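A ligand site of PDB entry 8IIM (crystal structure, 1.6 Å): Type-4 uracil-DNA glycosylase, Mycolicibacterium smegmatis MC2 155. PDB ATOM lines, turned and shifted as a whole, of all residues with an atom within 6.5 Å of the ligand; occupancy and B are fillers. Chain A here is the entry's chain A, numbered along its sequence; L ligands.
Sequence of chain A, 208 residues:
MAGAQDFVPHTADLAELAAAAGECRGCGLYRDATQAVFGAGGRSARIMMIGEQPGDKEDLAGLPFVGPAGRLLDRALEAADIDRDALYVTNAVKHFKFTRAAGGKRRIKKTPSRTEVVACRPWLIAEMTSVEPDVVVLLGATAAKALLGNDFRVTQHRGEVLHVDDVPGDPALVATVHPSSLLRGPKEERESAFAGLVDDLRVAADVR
Residues that only touch the ligand: Ala 4 (3.9 Å), Tyr 30 (3.8 Å), Lys 94 (3.7 Å) and Ala 119 (3.9 Å).
Ten residues have an atom within 4 Å of the ligand: Ala 4, Cys 24, Gly 26, Cys 27, Tyr 30, Lys 94, His 95, Ala 119, Cys 120 and Trp 123.
The backbone NH of Ala 36 is in hydrogen-bond range of a ring nitrogen (NE2) of His 95 (3.2 Å).
The backbone NH (N) of Lys 94 lies close to the side-chain sulfur (SG) of Cys 120, 3.5 Å away.
The backbone NH (N) of Leu 29 sits close to the side-chain sulfur (SG) of Cys 27, at 3.5 Å.
SG of Cys 24 lies close to N of Gly 26, 3.3 Å away.
The indole nitrogen of Trp 123 lies close to the side-chain sulfur of Cys 24, 3.4 Å away.
O of Ala 119 lies within hydrogen-bond range of N of Ala 4.
N of His 95 sits close to S3 of the ligand, at 3.7 Å.
A ring nitrogen (ND1) of His 95 is bound to an iron atom (FE4) of the ligand.
The side-chain sulfur of Cys 120 binds an iron atom (FE1) of the ligand (2.2 Å).
S1 of the ligand sits close to N of Cys 27, at 3.6 Å.
An iron atom (FE2) of the ligand is bound by the side-chain sulfur (SG) of Cys 27 (2.3 Å).
The side-chain sulfur of Cys 24 is bound to an iron atom (FE3) of the ligand.
S1 of the ligand sits close to N of Gly 26, at 3.6 Å.
The indole nitrogen (NE1) of Trp 123 lies close to a sulfur (S2) of the ligand, at 3.7 Å.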
ATOM      1  N   GLY A   3     -11.237 -30.123   2.545  1.00  0.00           N
ATOM      2  CA  GLY A   3     -11.232 -29.837   1.105  1.00  0.00           C
ATOM      3  C   GLY A   3     -11.721 -28.455   0.727  1.00  0.00           C
ATOM      4  O   GLY A   3     -11.331 -27.502   1.373  1.00  0.00           O
ATOM      5  N   ALA A   4     -12.550 -28.407  -0.311  1.00  0.00           N
ATOM      6  CA  ALA A   4     -13.028 -27.116  -0.845  1.00  0.00           C
ATOM      7  C   ALA A   4     -14.279 -26.606  -0.151  1.00  0.00           C
ATOM      8  O   ALA A   4     -14.729 -25.563  -0.527  1.00  0.00           O
ATOM      9  CB  ALA A   4     -13.419 -27.358  -2.283  1.00  0.00           C
ATOM     10  N   PHE A   7     -14.716 -22.952   0.678  1.00  0.00           N
ATOM     11  CA  PHE A   7     -14.589 -22.032  -0.436  1.00  0.00           C
ATOM     12  C   PHE A   7     -15.870 -21.945  -1.252  1.00  0.00           C
ATOM     13  O   PHE A   7     -15.968 -21.068  -2.116  1.00  0.00           O
ATOM     14  CB  PHE A   7     -13.424 -22.458  -1.337  1.00  0.00           C
ATOM     15  CG  PHE A   7     -12.080 -22.381  -0.664  1.00  0.00           C
ATOM     16  CD1 PHE A   7     -11.419 -21.169  -0.585  1.00  0.00           C
ATOM     17  CD2 PHE A   7     -11.495 -23.519  -0.116  1.00  0.00           C
ATOM     18  CE1 PHE A   7     -10.177 -21.090   0.050  1.00  0.00           C
ATOM     19  CE2 PHE A   7     -10.245 -23.442   0.525  1.00  0.00           C
ATOM     20  CZ  PHE A   7      -9.587 -22.220   0.595  1.00  0.00           C
ATOM     21  N   ALA A  21     -14.894 -20.425  -7.327  1.00  0.00           N
ATOM     22  CA  ALA A  21     -13.940 -21.508  -7.560  1.00  0.00           C
ATOM     23  C   ALA A  21     -12.587 -20.962  -8.002  1.00  0.00           C
ATOM     24  O   ALA A  21     -11.553 -21.590  -7.733  1.00  0.00           O
ATOM     25  CB  ALA A  21     -14.489 -22.496  -8.590  1.00  0.00           C
ATOM     26  N   CYS A  24     -10.457 -20.983  -5.017  1.00  0.00           N
ATOM     27  CA  CYS A  24     -10.382 -22.191  -4.203  1.00  0.00           C
ATOM     28  C   CYS A  24      -8.922 -22.588  -3.972  1.00  0.00           C
ATOM     29  O   CYS A  24      -8.105 -22.506  -4.892  1.00  0.00           O
ATOM     30  CB  CYS A  24     -11.130 -23.330  -4.895  1.00  0.00           C
ATOM     31  SG  CYS A  24     -11.220 -24.830  -3.915  1.00  0.00           S
ATOM     32  N   ARG A  25      -8.610 -22.977  -2.729  1.00  0.00           N
ATOM     33  CA  ARG A  25      -7.322 -23.596  -2.393  1.00  0.00           C
ATOM     34  C   ARG A  25      -7.550 -24.951  -1.710  1.00  0.00           C
ATOM     35  O   ARG A  25      -6.720 -25.397  -0.918  1.00  0.00           O
ATOM     36  CB  ARG A  25      -6.483 -22.675  -1.494  1.00  0.00           C
ATOM     37  CG  ARG A  25      -6.198 -21.293  -2.086  1.00  0.00           C
ATOM     38  CD  ARG A  25      -5.212 -20.506  -1.198  1.00  0.00           C
ATOM     39  NE  ARG A  25      -5.564 -20.567   0.231  1.00  0.00           N
ATOM     40  CZ  ARG A  25      -6.510 -19.817   0.777  1.00  0.00           C
ATOM     41  NH1 ARG A  25      -7.217 -18.966   0.039  1.00  0.00           N
ATOM     42  NH2 ARG A  25      -6.759 -19.921   2.071  1.00  0.00           N
ATOM     43  N   GLY A  26      -8.653 -25.633  -2.052  1.00  0.00           N
ATOM     44  CA  GLY A  26      -9.111 -26.826  -1.340  1.00  0.00           C
ATOM     45  C   GLY A  26      -8.188 -28.028  -1.452  1.00  0.00           C
ATOM     46  O   GLY A  26      -8.293 -28.955  -0.637  1.00  0.00           O
ATOM     47  N   CYS A  27      -7.329 -28.054  -2.458  1.00  0.00           N
ATOM     48  CA  CYS A  27      -6.240 -29.029  -2.529  1.00  0.00           C
ATOM     49  C   CYS A  27      -5.036 -28.313  -3.142  1.00  0.00           C
ATOM     50  O   CYS A  27      -5.042 -27.091  -3.299  1.00  0.00           O
ATOM     51  CB  CYS A  27      -6.700 -30.267  -3.313  1.00  0.00           C
ATOM     52  SG  CYS A  27      -6.810 -30.078  -5.120  1.00  0.00           S
ATOM     53  N   GLY A  28      -4.006 -29.066  -3.477  1.00  0.00           N
ATOM     54  CA  GLY A  28      -2.835 -28.373  -3.991  1.00  0.00           C
ATOM     55  C   GLY A  28      -2.891 -27.976  -5.456  1.00  0.00           C
ATOM     56  O   GLY A  28      -1.993 -27.264  -5.916  1.00  0.00           O
ATOM     57  N   LEU A  29      -3.899 -28.424  -6.200  1.00  0.00           N
ATOM     58  CA  LEU A  29      -3.812 -28.321  -7.659  1.00  0.00           C
ATOM     59  C   LEU A  29      -3.949 -26.890  -8.160  1.00  0.00           C
ATOM     60  O   LEU A  29      -3.552 -26.612  -9.299  1.00  0.00           O
ATOM     61  CB  LEU A  29      -4.874 -29.210  -8.310  1.00  0.00           C
ATOM     62  CG  LEU A  29      -4.677 -30.709  -8.014  1.00  0.00           C
ATOM     63  CD1 LEU A  29      -5.789 -31.511  -8.665  1.00  0.00           C
ATOM     64  CD2 LEU A  29      -3.324 -31.166  -8.547  1.00  0.00           C
ATOM     65  N   TYR A  30      -4.481 -25.971  -7.346  1.00  0.00           N
ATOM     66  CA  TYR A  30      -4.598 -24.599  -7.832  1.00  0.00           C
ATOM     67  C   TYR A  30      -3.237 -23.955  -8.073  1.00  0.00           C
ATOM     68  O   TYR A  30      -3.159 -22.988  -8.837  1.00  0.00           O
ATOM     69  CB  TYR A  30      -5.378 -23.733  -6.826  1.00  0.00           C
ATOM     70  CG  TYR A  30      -4.553 -23.364  -5.616  1.00  0.00           C
ATOM     71  CD1 TYR A  30      -4.432 -24.242  -4.546  1.00  0.00           C
ATOM     72  CD2 TYR A  30      -3.861 -22.143  -5.555  1.00  0.00           C
ATOM     73  CE1 TYR A  30      -3.663 -23.919  -3.436  1.00  0.00           C
ATOM     74  CE2 TYR A  30      -3.093 -21.810  -4.455  1.00  0.00           C
ATOM     75  CZ  TYR A  30      -3.012 -22.703  -3.393  1.00  0.00           C
ATOM     76  OH  TYR A  30      -2.227 -22.370  -2.298  1.00  0.00           O
ATOM     77  N   ARG A  31      -2.201 -24.458  -7.433  1.00  0.00           N
ATOM     78  CA  ARG A  31      -0.892 -23.743  -7.509  1.00  0.00           C
ATOM     79  C   ARG A  31      -0.306 -23.694  -8.921  1.00  0.00           C
ATOM     80  O   ARG A  31       0.078 -22.617  -9.370  1.00  0.00           O
ATOM     81  CB  ARG A  31       0.111 -24.386  -6.568  1.00  0.00           C
ATOM     82  CG  ARG A  31      -0.264 -24.295  -5.094  1.00  0.00           C
ATOM     83  CD  ARG A  31       0.978 -24.554  -4.256  1.00  0.00           C
ATOM     84  NE  ARG A  31       0.716 -24.565  -2.836  1.00  0.00           N
ATOM     85  CZ  ARG A  31       0.978 -23.549  -2.016  1.00  0.00           C
ATOM     86  NH1 ARG A  31       1.517 -22.438  -2.497  1.00  0.00           N
ATOM     87  NH2 ARG A  31       0.707 -23.645  -0.739  1.00  0.00           N
ATOM     88  N   ALA A  36      -8.907 -22.038 -12.375  1.00  0.00           N
ATOM     89  CA  ALA A  36      -9.950 -23.036 -12.226  1.00  0.00           C
ATOM     90  C   ALA A  36     -10.793 -23.054 -13.494  1.00  0.00           C
ATOM     91  O   ALA A  36     -10.992 -22.016 -14.125  1.00  0.00           O
ATOM     92  CB  ALA A  36     -10.835 -22.733 -11.015  1.00  0.00           C
ATOM     93  N   ALA A  92     -14.664 -33.609 -12.539  1.00  0.00           N
ATOM     94  CA  ALA A  92     -14.615 -33.998 -11.127  1.00  0.00           C
ATOM     95  C   ALA A  92     -13.678 -33.093 -10.344  1.00  0.00           C
ATOM     96  O   ALA A  92     -13.954 -32.765  -9.176  1.00  0.00           O
ATOM     97  CB  ALA A  92     -14.191 -35.462 -11.006  1.00  0.00           C
ATOM     98  N   VAL A  93     -12.538 -32.714 -10.940  1.00  0.00           N
ATOM     99  CA  VAL A  93     -11.673 -31.731 -10.298  1.00  0.00           C
ATOM    100  C   VAL A  93     -11.522 -30.553 -11.263  1.00  0.00           C
ATOM    101  O   VAL A  93     -11.638 -30.734 -12.487  1.00  0.00           O
ATOM    102  CB  VAL A  93     -10.301 -32.300  -9.863  1.00  0.00           C
ATOM    103  CG1 VAL A  93     -10.456 -33.555  -8.961  1.00  0.00           C
ATOM    104  CG2 VAL A  93      -9.421 -32.602 -11.050  1.00  0.00           C
ATOM    105  N   LYS A  94     -11.340 -29.355 -10.713  1.00  0.00           N
ATOM    106  CA  LYS A  94     -11.434 -28.103 -11.517  1.00  0.00           C
ATOM    107  C   LYS A  94     -10.101 -27.458 -11.856  1.00  0.00           C
ATOM    108  O   LYS A  94     -10.112 -26.457 -12.541  1.00  0.00           O
ATOM    109  CB  LYS A  94     -12.220 -27.105 -10.662  1.00  0.00           C
ATOM    110  CG  LYS A  94     -13.699 -26.931 -10.986  1.00  0.00           C
ATOM    111  CD  LYS A  94     -14.457 -28.197 -10.932  1.00  0.00           C
ATOM    112  CE  LYS A  94     -15.960 -27.982 -10.970  1.00  0.00           C
ATOM    113  NZ  LYS A  94     -16.627 -29.291 -10.782  1.00  0.00           N
ATOM    114  N   HIS A  95      -9.019 -28.053 -11.381  1.00  0.00           N
ATOM    115  CA  HIS A  95      -7.686 -27.568 -11.757  1.00  0.00           C
ATOM    116  C   HIS A  95      -6.903 -28.685 -12.476  1.00  0.00           C
ATOM    117  O   HIS A  95      -6.924 -29.798 -12.035  1.00  0.00           O
ATOM    118  CB  HIS A  95      -6.878 -27.012 -10.594  1.00  0.00           C
ATOM    119  CG  HIS A  95      -7.241 -25.630 -10.192  1.00  0.00           C
ATOM    120  ND1 HIS A  95      -8.076 -25.387  -9.155  1.00  0.00           N
ATOM    121  CD2 HIS A  95      -6.877 -24.433 -10.665  1.00  0.00           C
ATOM    122  CE1 HIS A  95      -8.215 -24.099  -8.963  1.00  0.00           C
ATOM    123  NE2 HIS A  95      -7.487 -23.497  -9.877  1.00  0.00           N
ATOM    124  N   PHE A  96      -6.214 -28.303 -13.537  1.00  0.00           N
ATOM    125  CA  PHE A  96      -5.420 -29.229 -14.336  1.00  0.00           C
ATOM    126  C   PHE A  96      -4.190 -29.685 -13.553  1.00  0.00           C
ATOM    127  O   PHE A  96      -3.440 -28.860 -13.035  1.00  0.00           O
ATOM    128  CB  PHE A  96      -5.012 -28.476 -15.615  1.00  0.00           C
ATOM    129  CG  PHE A  96      -4.137 -29.234 -16.577  1.00  0.00           C
ATOM    130  CD1 PHE A  96      -4.320 -30.582 -16.856  1.00  0.00           C
ATOM    131  CD2 PHE A  96      -3.163 -28.523 -17.302  1.00  0.00           C
ATOM    132  CE1 PHE A  96      -3.513 -31.232 -17.801  1.00  0.00           C
ATOM    133  CE2 PHE A  96      -2.355 -29.159 -18.243  1.00  0.00           C
ATOM    134  CZ  PHE A  96      -2.539 -30.513 -18.505  1.00  0.00           C
ATOM    135  N   GLU A 116      -7.671 -35.730  -3.818  1.00  0.00           N
ATOM    136  CA  GLU A 116      -8.027 -34.538  -4.584  1.00  0.00           C
ATOM    137  C   GLU A 116      -9.472 -34.566  -5.072  1.00  0.00           C
ATOM    138  O   GLU A 116     -10.175 -33.558  -5.024  1.00  0.00           O
ATOM    139  CB  GLU A 116      -7.057 -34.366  -5.760  1.00  0.00           C
ATOM    140  CG  GLU A 116      -5.681 -33.862  -5.275  1.00  0.00           C
ATOM    141  CD  GLU A 116      -4.519 -34.197  -6.182  1.00  0.00           C
ATOM    142  OE1 GLU A 116      -4.645 -35.040  -7.099  1.00  0.00           O
ATOM    143  OE2 GLU A 116      -3.431 -33.597  -5.960  1.00  0.00           O
ATOM    144  N   ALA A 119     -11.621 -33.825  -2.192  1.00  0.00           N
ATOM    145  CA  ALA A 119     -11.480 -32.417  -1.817  1.00  0.00           C
ATOM    146  C   ALA A 119     -12.309 -31.526  -2.718  1.00  0.00           C
ATOM    147  O   ALA A 119     -12.896 -30.546  -2.258  1.00  0.00           O
ATOM    148  CB  ALA A 119     -10.004 -32.004  -1.870  1.00  0.00           C
ATOM    149  N   CYS A 120     -12.358 -31.842  -4.020  1.00  0.00           N
ATOM    150  CA  CYS A 120     -13.024 -30.953  -4.961  1.00  0.00           C
ATOM    151  C   CYS A 120     -14.521 -31.239  -5.062  1.00  0.00           C
ATOM    152  O   CYS A 120     -15.273 -30.409  -5.600  1.00  0.00           O
ATOM    153  CB  CYS A 120     -12.366 -31.108  -6.337  1.00  0.00           C
ATOM    154  SG  CYS A 120     -12.599 -29.663  -7.450  1.00  0.00           S
ATOM    155  N   ARG A 121     -14.950 -32.387  -4.551  1.00  0.00           N
ATOM    156  CA  ARG A 121     -16.325 -32.816  -4.752  1.00  0.00           C
ATOM    157  C   ARG A 121     -17.358 -31.810  -4.235  1.00  0.00           C
ATOM    158  O   ARG A 121     -18.438 -31.760  -4.851  1.00  0.00           O
ATOM    159  CB  ARG A 121     -16.535 -34.200  -4.106  1.00  0.00           C
ATOM    160  CG  ARG A 121     -17.830 -34.887  -4.556  1.00  0.00           C
ATOM    161  CD  ARG A 121     -17.735 -36.375  -4.278  1.00  0.00           C
ATOM    162  NE  ARG A 121     -17.509 -36.587  -2.863  1.00  0.00           N
ATOM    163  CZ  ARG A 121     -17.214 -37.765  -2.333  1.00  0.00           C
ATOM    164  NH1 ARG A 121     -17.093 -38.849  -3.083  1.00  0.00           N
ATOM    165  NH2 ARG A 121     -17.011 -37.850  -1.017  1.00  0.00           N
ATOM    166  N   TRP A 123     -17.607 -28.795  -5.003  1.00  0.00           N
ATOM    167  CA  TRP A 123     -18.014 -28.022  -6.174  1.00  0.00           C
ATOM    168  C   TRP A 123     -18.994 -28.808  -7.019  1.00  0.00           C
ATOM    169  O   TRP A 123     -20.000 -28.266  -7.495  1.00  0.00           O
ATOM    170  CB  TRP A 123     -16.801 -27.626  -7.023  1.00  0.00           C
ATOM    171  CG  TRP A 123     -15.919 -26.625  -6.344  1.00  0.00           C
ATOM    172  CD1 TRP A 123     -14.615 -26.832  -5.931  1.00  0.00           C
ATOM    173  CD2 TRP A 123     -16.252 -25.280  -5.980  1.00  0.00           C
ATOM    174  NE1 TRP A 123     -14.138 -25.685  -5.328  1.00  0.00           N
ATOM    175  CE2 TRP A 123     -15.113 -24.723  -5.339  1.00  0.00           C
ATOM    176  CE3 TRP A 123     -17.401 -24.484  -6.112  1.00  0.00           C
ATOM    177  CZ2 TRP A 123     -15.086 -23.415  -4.845  1.00  0.00           C
ATOM    178  CZ3 TRP A 123     -17.381 -23.160  -5.620  1.00  0.00           C
ATOM    179  CH2 TRP A 123     -16.228 -22.655  -4.986  1.00  0.00           C
HETATM  180 FE1  LIG L   1     -10.840 -28.407  -6.835  1.00  0.00          FE
HETATM  181 FE2  LIG L   1      -8.416 -28.520  -5.626  1.00  0.00          FE
HETATM  182 FE3  LIG L   1     -10.117 -26.379  -5.215  1.00  0.00          FE
HETATM  183 FE4  LIG L   1      -8.841 -26.733  -7.552  1.00  0.00          FE
HETATM  184  S1  LIG L   1      -7.848 -26.287  -5.531  1.00  0.00           S
HETATM  185  S2  LIG L   1     -11.084 -26.187  -7.307  1.00  0.00           S
HETATM  186  S3  LIG L   1      -8.875 -28.971  -7.841  1.00  0.00           S
HETATM  187  S4  LIG L   1     -10.429 -28.549  -4.569  1.00  0.00           S
